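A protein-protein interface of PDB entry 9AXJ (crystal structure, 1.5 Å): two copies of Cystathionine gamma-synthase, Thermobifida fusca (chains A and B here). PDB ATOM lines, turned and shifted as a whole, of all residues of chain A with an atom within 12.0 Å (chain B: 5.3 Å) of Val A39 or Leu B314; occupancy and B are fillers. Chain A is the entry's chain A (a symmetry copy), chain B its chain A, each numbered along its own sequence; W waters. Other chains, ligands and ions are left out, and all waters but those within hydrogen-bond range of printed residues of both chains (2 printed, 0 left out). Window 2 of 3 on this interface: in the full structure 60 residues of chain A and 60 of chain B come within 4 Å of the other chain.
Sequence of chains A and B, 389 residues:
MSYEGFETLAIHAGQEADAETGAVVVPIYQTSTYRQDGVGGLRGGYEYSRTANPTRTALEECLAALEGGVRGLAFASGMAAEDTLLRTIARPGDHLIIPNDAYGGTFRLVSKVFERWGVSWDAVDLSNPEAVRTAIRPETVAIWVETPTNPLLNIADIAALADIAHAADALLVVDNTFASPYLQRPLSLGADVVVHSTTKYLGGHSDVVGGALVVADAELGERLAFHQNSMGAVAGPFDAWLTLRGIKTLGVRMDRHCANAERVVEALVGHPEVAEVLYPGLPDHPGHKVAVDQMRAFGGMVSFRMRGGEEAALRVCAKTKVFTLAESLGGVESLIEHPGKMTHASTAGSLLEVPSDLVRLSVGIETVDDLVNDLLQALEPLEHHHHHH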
ATOM      1  N   THR A  33     -15.468 -11.396  -0.122  1.00  0.00           N
ATOM      2  CA  THR A  33     -16.102 -12.567   0.532  1.00  0.00           C
ATOM      3  C   THR A  33     -15.909 -13.830  -0.271  1.00  0.00           C
ATOM      4  O   THR A  33     -15.294 -13.783  -1.396  1.00  0.00           O
ATOM      5  CB  THR A  33     -17.573 -12.240   0.825  1.00  0.00           C
ATOM      6  OG1 THR A  33     -18.054 -13.221   1.753  1.00  0.00           O
ATOM      7  CG2 THR A  33     -18.444 -12.148  -0.424  1.00  0.00           C
ATOM      8  N   TYR A  34     -16.366 -14.923   0.291  1.00  0.00           N
ATOM      9  CA  TYR A  34     -15.995 -16.312  -0.123  1.00  0.00           C
ATOM     10  C   TYR A  34     -17.204 -17.199   0.032  1.00  0.00           C
ATOM     11  O   TYR A  34     -17.845 -17.208   1.090  1.00  0.00           O
ATOM     12  CB  TYR A  34     -14.828 -16.850   0.703  1.00  0.00           C
ATOM     13  CG  TYR A  34     -13.638 -15.911   0.721  1.00  0.00           C
ATOM     14  CD1 TYR A  34     -13.597 -14.807   1.572  1.00  0.00           C
ATOM     15  CD2 TYR A  34     -12.551 -16.118  -0.088  1.00  0.00           C
ATOM     16  CE1 TYR A  34     -12.517 -13.937   1.572  1.00  0.00           C
ATOM     17  CE2 TYR A  34     -11.474 -15.274  -0.125  1.00  0.00           C
ATOM     18  CZ  TYR A  34     -11.464 -14.151   0.673  1.00  0.00           C
ATOM     19  OH  TYR A  34     -10.435 -13.232   0.604  1.00  0.00           O
ATOM     20  N   ARG A  35     -17.507 -17.952  -1.004  1.00  0.00           N
ATOM     21  CA  ARG A  35     -18.589 -18.916  -0.985  1.00  0.00           C
ATOM     22  C   ARG A  35     -18.268 -20.042  -0.005  1.00  0.00           C
ATOM     23  O   ARG A  35     -17.170 -20.550   0.005  1.00  0.00           O
ATOM     24  CB  ARG A  35     -18.742 -19.553  -2.367  1.00  0.00           C
ATOM     25  CG  ARG A  35     -19.838 -20.626  -2.421  1.00  0.00           C
ATOM     26  CD  ARG A  35     -19.936 -21.171  -3.847  1.00  0.00           C
ATOM     27  NE  ARG A  35     -20.751 -22.342  -3.886  1.00  0.00           N
ATOM     28  CZ  ARG A  35     -20.973 -23.021  -5.008  1.00  0.00           C
ATOM     29  NH1 ARG A  35     -21.690 -24.133  -4.973  1.00  0.00           N
ATOM     30  NH2 ARG A  35     -20.538 -22.511  -6.167  1.00  0.00           N
ATOM     31  N   GLN A  36     -19.230 -20.421   0.816  1.00  0.00           N
ATOM     32  CA  GLN A  36     -19.147 -21.533   1.788  1.00  0.00           C
ATOM     33  C   GLN A  36     -19.979 -22.706   1.273  1.00  0.00           C
ATOM     34  O   GLN A  36     -21.039 -22.510   0.660  1.00  0.00           O
ATOM     35  CB  GLN A  36     -19.666 -21.073   3.154  1.00  0.00           C
ATOM     36  CG  GLN A  36     -18.893 -19.870   3.688  1.00  0.00           C
ATOM     37  CD  GLN A  36     -19.249 -19.480   5.099  1.00  0.00           C
ATOM     38  OE1 GLN A  36     -19.737 -20.324   5.890  1.00  0.00           O
ATOM     39  NE2 GLN A  36     -18.884 -18.230   5.467  1.00  0.00           N
ATOM     40  N   ASP A  37     -19.507 -23.919   1.526  1.00  0.00           N
ATOM     41  CA  ASP A  37     -20.188 -25.157   1.118  1.00  0.00           C
ATOM     42  C   ASP A  37     -21.077 -25.623   2.300  1.00  0.00           C
ATOM     43  O   ASP A  37     -20.632 -26.386   3.196  1.00  0.00           O
ATOM     44  CB  ASP A  37     -19.187 -26.217   0.680  1.00  0.00           C
ATOM     45  CG  ASP A  37     -18.365 -25.714  -0.508  1.00  0.00           C
ATOM     46  OD1 ASP A  37     -19.017 -25.383  -1.506  1.00  0.00           O
ATOM     47  OD2 ASP A  37     -17.149 -25.789  -0.433  1.00  0.00           O
ATOM     48  N   GLY A  38     -22.285 -25.105   2.319  1.00  0.00           N
ATOM     49  CA  GLY A  38     -23.156 -25.181   3.509  1.00  0.00           C
ATOM     50  C   GLY A  38     -22.659 -24.167   4.549  1.00  0.00           C
ATOM     51  O   GLY A  38     -21.521 -23.662   4.495  1.00  0.00           O
ATOM     52  N   VAL A  39     -23.520 -23.841   5.488  1.00  0.00           N
ATOM     53  CA  VAL A  39     -23.171 -22.827   6.509  1.00  0.00           C
ATOM     54  C   VAL A  39     -21.968 -23.315   7.334  1.00  0.00           C
ATOM     55  O   VAL A  39     -22.078 -24.379   7.946  1.00  0.00           O
ATOM     56  CB  VAL A  39     -24.416 -22.563   7.376  1.00  0.00           C
ATOM     57  CG1 VAL A  39     -24.047 -21.710   8.564  1.00  0.00           C
ATOM     58  CG2 VAL A  39     -25.497 -21.901   6.534  1.00  0.00           C
ATOM     59  N   GLY A  40     -20.898 -22.531   7.371  1.00  0.00           N
ATOM     60  CA  GLY A  40     -19.634 -22.862   8.070  1.00  0.00           C
ATOM     61  C   GLY A  40     -18.740 -23.795   7.282  1.00  0.00           C
ATOM     62  O   GLY A  40     -17.637 -24.156   7.798  1.00  0.00           O
ATOM     63  N   GLY A  41     -19.124 -24.191   6.048  1.00  0.00           N
ATOM     64  CA  GLY A  41     -18.277 -25.058   5.216  1.00  0.00           C
ATOM     65  C   GLY A  41     -17.221 -24.234   4.519  1.00  0.00           C
ATOM     66  O   GLY A  41     -17.338 -24.063   3.271  1.00  0.00           O
ATOM     67  N   LEU A  42     -16.158 -23.809   5.233  1.00  0.00           N
ATOM     68  CA  LEU A  42     -15.238 -22.823   4.615  1.00  0.00           C
ATOM     69  C   LEU A  42     -14.413 -23.543   3.561  1.00  0.00           C
ATOM     70  O   LEU A  42     -14.118 -24.730   3.708  1.00  0.00           O
ATOM     71  CB  LEU A  42     -14.331 -22.187   5.643  1.00  0.00           C
ATOM     72  CG  LEU A  42     -15.060 -21.484   6.793  1.00  0.00           C
ATOM     73  CD1 LEU A  42     -14.073 -20.718   7.633  1.00  0.00           C
ATOM     74  CD2 LEU A  42     -16.156 -20.602   6.296  1.00  0.00           C
ATOM     75  N   ARG A  43     -14.151 -22.868   2.476  1.00  0.00           N
ATOM     76  CA  ARG A  43     -13.179 -23.360   1.495  1.00  0.00           C
ATOM     77  C   ARG A  43     -11.806 -22.812   1.803  1.00  0.00           C
ATOM     78  O   ARG A  43     -11.622 -21.533   1.763  1.00  0.00           O
ATOM     79  CB  ARG A  43     -13.513 -22.835   0.109  1.00  0.00           C
ATOM     80  CG  ARG A  43     -14.758 -23.402  -0.429  1.00  0.00           C
ATOM     81  CD  ARG A  43     -15.005 -23.012  -1.846  1.00  0.00           C
ATOM     82  NE  ARG A  43     -16.186 -23.736  -2.328  1.00  0.00           N
ATOM     83  CZ  ARG A  43     -16.621 -23.661  -3.580  1.00  0.00           C
ATOM     84  NH1 ARG A  43     -16.038 -22.808  -4.435  1.00  0.00           N
ATOM     85  NH2 ARG A  43     -17.726 -24.304  -3.897  1.00  0.00           N
ATOM     86  N   GLY A  45     -10.428 -22.385   4.412  1.00  0.00           N
ATOM     87  CA  GLY A  45     -10.388 -21.606   5.649  1.00  0.00           C
ATOM     88  C   GLY A  45     -10.777 -20.145   5.448  1.00  0.00           C
ATOM     89  O   GLY A  45     -10.744 -19.391   6.467  1.00  0.00           O
ATOM     90  N   TYR A  46     -11.272 -19.747   4.277  1.00  0.00           N
ATOM     91  CA  TYR A  46     -11.593 -18.327   4.022  1.00  0.00           C
ATOM     92  C   TYR A  46     -13.081 -18.050   4.173  1.00  0.00           C
ATOM     93  O   TYR A  46     -13.946 -18.896   3.865  1.00  0.00           O
ATOM     94  CB  TYR A  46     -11.096 -17.908   2.626  1.00  0.00           C
ATOM     95  CG  TYR A  46      -9.592 -17.829   2.614  1.00  0.00           C
ATOM     96  CD1 TYR A  46      -8.965 -16.717   3.188  1.00  0.00           C
ATOM     97  CD2 TYR A  46      -8.771 -18.863   2.178  1.00  0.00           C
ATOM     98  CE1 TYR A  46      -7.606 -16.618   3.305  1.00  0.00           C
ATOM     99  CE2 TYR A  46      -7.381 -18.781   2.297  1.00  0.00           C
ATOM    100  CZ  TYR A  46      -6.779 -17.658   2.871  1.00  0.00           C
ATOM    101  OH  TYR A  46      -5.410 -17.610   3.029  1.00  0.00           O
ATOM    102  N   GLU A  47     -13.383 -16.854   4.663  1.00  0.00           N
ATOM    103  CA  GLU A  47     -14.779 -16.458   4.939  1.00  0.00           C
ATOM    104  C   GLU A  47     -15.021 -14.992   4.647  1.00  0.00           C
ATOM    105  O   GLU A  47     -16.131 -14.640   4.164  1.00  0.00           O
ATOM    106  CB  GLU A  47     -15.219 -16.844   6.346  1.00  0.00           C
ATOM    107  CG  GLU A  47     -14.511 -16.200   7.466  1.00  0.00           C
ATOM    108  CD  GLU A  47     -14.870 -16.708   8.860  1.00  0.00           C
ATOM    109  OE1 GLU A  47     -15.948 -17.193   9.062  1.00  0.00           O
ATOM    110  OE2 GLU A  47     -14.006 -16.715   9.650  1.00  0.00           O
ATOM    111  N   GLY B 309     -37.626 -23.910  11.562  1.00  0.00           N
ATOM    112  CA  GLY B 309     -36.590 -23.648  12.556  1.00  0.00           C
ATOM    113  C   GLY B 309     -35.197 -23.524  11.935  1.00  0.00           C
ATOM    114  O   GLY B 309     -35.070 -23.419  10.691  1.00  0.00           O
ATOM    115  N   GLU B 310     -34.209 -23.673  12.773  1.00  0.00           N
ATOM    116  CA  GLU B 310     -32.787 -23.587  12.371  1.00  0.00           C
ATOM    117  C   GLU B 310     -32.530 -24.616  11.264  1.00  0.00           C
ATOM    118  O   GLU B 310     -31.814 -24.313  10.311  1.00  0.00           O
ATOM    119  CB  GLU B 310     -31.883 -23.835  13.556  1.00  0.00           C
ATOM    120  CG  GLU B 310     -30.407 -23.673  13.234  1.00  0.00           C
ATOM    121  CD  GLU B 310     -29.460 -23.967  14.380  1.00  0.00           C
ATOM    122  OE1 GLU B 310     -29.148 -25.116  14.578  1.00  0.00           O
ATOM    123  OE2 GLU B 310     -29.024 -23.017  15.037  1.00  0.00           O
ATOM    124  N   GLU B 311     -33.023 -25.848  11.435  1.00  0.00           N
ATOM    125  CA  GLU B 311     -32.756 -26.932  10.474  1.00  0.00           C
ATOM    126  C   GLU B 311     -33.195 -26.461   9.076  1.00  0.00           C
ATOM    127  O   GLU B 311     -32.415 -26.639   8.122  1.00  0.00           O
ATOM    128  CB  GLU B 311     -33.452 -28.187  11.006  1.00  0.00           C
ATOM    129  CG  GLU B 311     -33.404 -29.388  10.122  1.00  0.00           C
ATOM    130  CD  GLU B 311     -34.202 -30.564  10.740  1.00  0.00           C
ATOM    131  OE1 GLU B 311     -35.417 -30.432  10.950  1.00  0.00           O
ATOM    132  OE2 GLU B 311     -33.589 -31.531  11.138  1.00  0.00           O
ATOM    133  N   ALA B 312     -34.378 -25.875   8.940  1.00  0.00           N
ATOM    134  CA  ALA B 312     -34.935 -25.445   7.641  1.00  0.00           C
ATOM    135  C   ALA B 312     -34.119 -24.279   7.106  1.00  0.00           C
ATOM    136  O   ALA B 312     -33.860 -24.225   5.884  1.00  0.00           O
ATOM    137  CB  ALA B 312     -36.422 -25.091   7.767  1.00  0.00           C
ATOM    138  N   ALA B 313     -33.770 -23.334   7.963  1.00  0.00           N
ATOM    139  CA  ALA B 313     -32.963 -22.153   7.518  1.00  0.00           C
ATOM    140  C   ALA B 313     -31.608 -22.612   6.945  1.00  0.00           C
ATOM    141  O   ALA B 313     -31.178 -22.031   5.926  1.00  0.00           O
ATOM    142  CB  ALA B 313     -32.766 -21.159   8.653  1.00  0.00           C
ATOM    143  N   LEU B 314     -30.906 -23.498   7.618  1.00  0.00           N
ATOM    144  CA  LEU B 314     -29.599 -23.977   7.150  1.00  0.00           C
ATOM    145  C   LEU B 314     -29.774 -24.699   5.805  1.00  0.00           C
ATOM    146  O   LEU B 314     -28.902 -24.525   4.931  1.00  0.00           O
ATOM    147  CB  LEU B 314     -28.932 -24.882   8.173  1.00  0.00           C
ATOM    148  CG  LEU B 314     -28.619 -24.260   9.535  1.00  0.00           C
ATOM    149  CD1 LEU B 314     -28.057 -25.314  10.497  1.00  0.00           C
ATOM    150  CD2 LEU B 314     -27.710 -23.084   9.406  1.00  0.00           C
ATOM    151  N   ARG B 315     -30.856 -25.415   5.633  1.00  0.00           N
ATOM    152  CA  ARG B 315     -31.104 -26.142   4.342  1.00  0.00           C
ATOM    153  C   ARG B 315     -31.302 -25.156   3.209  1.00  0.00           C
ATOM    154  O   ARG B 315     -30.650 -25.336   2.155  1.00  0.00           O
ATOM    155  CB  ARG B 315     -32.313 -27.069   4.383  1.00  0.00           C
ATOM    156  CG  ARG B 315     -31.936 -28.433   4.898  1.00  0.00           C
ATOM    157  CD  ARG B 315     -33.088 -29.432   4.726  1.00  0.00           C
ATOM    158  NE  ARG B 315     -34.384 -28.765   4.735  1.00  0.00           N
ATOM    159  CZ  ARG B 315     -35.251 -28.758   5.752  1.00  0.00           C
ATOM    160  NH1 ARG B 315     -36.412 -28.144   5.567  1.00  0.00           N
ATOM    161  NH2 ARG B 315     -34.980 -29.378   6.917  1.00  0.00           N
ATOM    162  N   VAL B 316     -32.072 -24.075   3.436  1.00  0.00           N
ATOM    163  CA  VAL B 316     -32.302 -23.065   2.368  1.00  0.00           C
ATOM    164  C   VAL B 316     -30.942 -22.455   1.962  1.00  0.00           C
ATOM    165  O   VAL B 316     -30.624 -22.304   0.767  1.00  0.00           O
ATOM    166  CB  VAL B 316     -33.308 -21.996   2.835  1.00  0.00           C
ATOM    167  CG1 VAL B 316     -33.398 -20.902   1.800  1.00  0.00           C
ATOM    168  CG2 VAL B 316     -34.658 -22.575   3.088  1.00  0.00           C
ATOM    169  N   CYS B 317     -30.167 -22.040   2.957  1.00  0.00           N
ATOM    170  CA  CYS B 317     -28.874 -21.415   2.747  1.00  0.00           C
ATOM    171  C   CYS B 317     -28.003 -22.291   1.821  1.00  0.00           C
ATOM    172  O   CYS B 317     -27.225 -21.706   1.059  1.00  0.00           O
ATOM    173  CB  CYS B 317     -28.175 -21.179   4.079  1.00  0.00           C
ATOM    174  SG  CYS B 317     -28.855 -19.765   4.954  1.00  0.00           S
ATOM    175  N   ALA B 318     -28.016 -23.604   1.998  1.00  0.00           N
ATOM    176  CA  ALA B 318     -27.139 -24.546   1.255  1.00  0.00           C
ATOM    177  C   ALA B 318     -27.647 -24.832  -0.152  1.00  0.00           C
ATOM    178  O   ALA B 318     -26.878 -25.400  -0.916  1.00  0.00           O
ATOM    179  CB  ALA B 318     -26.996 -25.815   2.000  1.00  0.00           C
ATOM    180  N   LEU B 325     -23.912 -18.457  -0.972  1.00  0.00           N
ATOM    181  CA  LEU B 325     -23.824 -18.530   0.504  1.00  0.00           C
ATOM    182  C   LEU B 325     -22.464 -17.974   0.936  1.00  0.00           C
ATOM    183  O   LEU B 325     -21.426 -18.567   0.650  1.00  0.00           O
ATOM    184  CB  LEU B 325     -23.938 -19.975   0.954  1.00  0.00           C
ATOM    185  CG  LEU B 325     -23.833 -20.216   2.472  1.00  0.00           C
ATOM    186  CD1 LEU B 325     -24.840 -19.421   3.213  1.00  0.00           C
ATOM    187  CD2 LEU B 325     -23.990 -21.702   2.738  1.00  0.00           C
ATOM    188  N   HIS B 338     -26.819 -17.230   6.968  1.00  0.00           N
ATOM    189  CA  HIS B 338     -27.459 -17.521   8.263  1.00  0.00           C
ATOM    190  C   HIS B 338     -26.762 -16.665   9.306  1.00  0.00           C
ATOM    191  O   HIS B 338     -25.664 -16.997   9.736  1.00  0.00           O
ATOM    192  CB  HIS B 338     -27.327 -18.986   8.549  1.00  0.00           C
ATOM    193  CG  HIS B 338     -28.015 -19.373   9.802  1.00  0.00           C
ATOM    194  ND1 HIS B 338     -27.357 -19.458  11.020  1.00  0.00           N
ATOM    195  CD2 HIS B 338     -29.322 -19.718  10.008  1.00  0.00           C
ATOM    196  CE1 HIS B 338     -28.253 -19.839  11.912  1.00  0.00           C
ATOM    197  NE2 HIS B 338     -29.438 -20.038  11.334  1.00  0.00           N
ATOM    198  N   LYS B 341     -25.115 -18.240  12.707  1.00  0.00           N
ATOM    199  CA  LYS B 341     -23.845 -19.012  12.640  1.00  0.00           C
ATOM    200  C   LYS B 341     -22.742 -18.287  11.833  1.00  0.00           C
ATOM    201  O   LYS B 341     -21.565 -18.722  11.924  1.00  0.00           O
ATOM    202  CB  LYS B 341     -24.132 -20.377  12.039  1.00  0.00           C
ATOM    203  CG  LYS B 341     -24.850 -21.326  12.992  1.00  0.00           C
ATOM    204  CD  LYS B 341     -25.299 -22.604  12.339  1.00  0.00           C
ATOM    205  CE  LYS B 341     -25.369 -23.838  13.223  1.00  0.00           C
ATOM    206  NZ  LYS B 341     -25.561 -23.535  14.644  1.00  0.00           N
ATOM    207  N   MET B 342     -23.071 -17.215  11.158  1.00  0.00           N
ATOM    208  CA  MET B 342     -22.139 -16.483  10.259  1.00  0.00           C
ATOM    209  C   MET B 342     -21.912 -15.075  10.823  1.00  0.00           C
ATOM    210  O   MET B 342     -21.152 -14.978  11.828  1.00  0.00           O
ATOM    211  CB  MET B 342     -22.621 -16.559   8.803  1.00  0.00           C
ATOM    212  CG  MET B 342     -22.672 -18.012   8.286  1.00  0.00           C
ATOM    213  SD  MET B 342     -23.431 -18.276   6.679  1.00  0.00           S
ATOM    214  CE  MET B 342     -22.340 -17.318   5.617  1.00  0.00           C
HETATM  215  O   HOH W   1     -24.007 -24.614  -0.318  1.00  0.00           O
HETATM  216  O   HOH W   2     -26.168 -25.044   5.436  1.00  0.00           O
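Printed residues of chain A that touch a printed residue of chain B: Tyr A34, Arg A35, Gln A36, Gly A38 and Val A39.
Printed residues of chain B that touch a printed residue of chain A: Leu B314, Cys B317, Leu B325, His B338, Lys B341 and Met B342.
Hydrophobic or aromatic side chains of chain B that line the printed part of chain A: Leu B314, Leu B325, His B338 and Met B342.
Among the printed residues, no Asp or Glu carboxylate lies within 4 Å of a Lys or Arg side-chain nitrogen of the other chain.
Printed residues of chain B within 4 Å of Val A39: Leu B314 (3.8 Å), Cys B317 (3.7 Å), Leu B325 (3.5 Å), His B338 (3.99 Å), Lys B341 (3.7 Å) and Met B342 (3.96 Å).
Leu B314 touches just one residue of chain A: Val A39.
No residue of chain A comes within 4 Å of Gly B309.
No residue of chain A comes within 4 Å of Glu B310.
Ala B313 touches none of the printed residues of chain A.
No residue of chain A comes within 4 Å of Arg B315.
No residue of chain A comes within 4 Å of Val B316.
Cys B317 touches just one residue of chain A: Val A39 (3.7 Å).
No residue of chain A comes within 4 Å of Ala B318.
Of chain A, only Val A39 comes within 4 Å of Lys B341.
Printed residues of chain B within 4 Å of Tyr A34: Leu B325.
Printed residues of chain B within 4 Å of Gln A36: Leu B325 (2.9 Å) and Met B342 (3.6 Å).
Gly A41 touches none of the printed residues of chain B.
The nearest printed residue of chain B that does not touch Val A39 is Ala B318 (5.3 Å).
The backbone NH of Gln A36 lies within hydrogen-bond range of the backbone carbonyl oxygen of Leu B325, at 2.9 Å.
Water W2 bridges the backbone carbonyl oxygen of Leu B314 and the backbone NH of Val A39.
Water W1 bridges O of Ala B318 (3.0 Å) and N of Gly A38 (3.2 Å).
No position is printed for both chains.
Of the 11 pairs that touch across the chains among the printed residues, none has its exchanged pair printed and touching as well.
Among the printed residues, merely in contact across the chains: Arg A35 with Leu B325, Gly A38 with Leu B325, Val A39 with Leu B325, Gln A36 with Met B342, Val A39 with Cys B317, Val A39 with Lys B341, Val A39 with Leu B314, Tyr A34 with Leu B325, Val A39 with Met B342 and Val A39 with His B338.
The side-chain amino group (NZ) of Lys B341 is in salt-bridge range of the side-chain carboxylate (OE2) of Glu B310, at 3.5 Å.
The backbone carbonyl oxygen (O) of Ala B313 is in hydrogen-bond range of the side-chain sulfur (SG) of Cys B317, 3.4 Å away.
A ring nitrogen (ND1) of His B338 is in hydrogen-bond range of the backbone NH (N) of Lys B341 (3.1 Å).
The backbone NH (N) of His B338 lies within hydrogen-bond range of the side-chain sulfur (SD) of Met B342 (3.6 Å).
The side-chain amide oxygen (OE1) of Gln A36 is in hydrogen-bond range of the backbone NH (N) of Gly A40.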
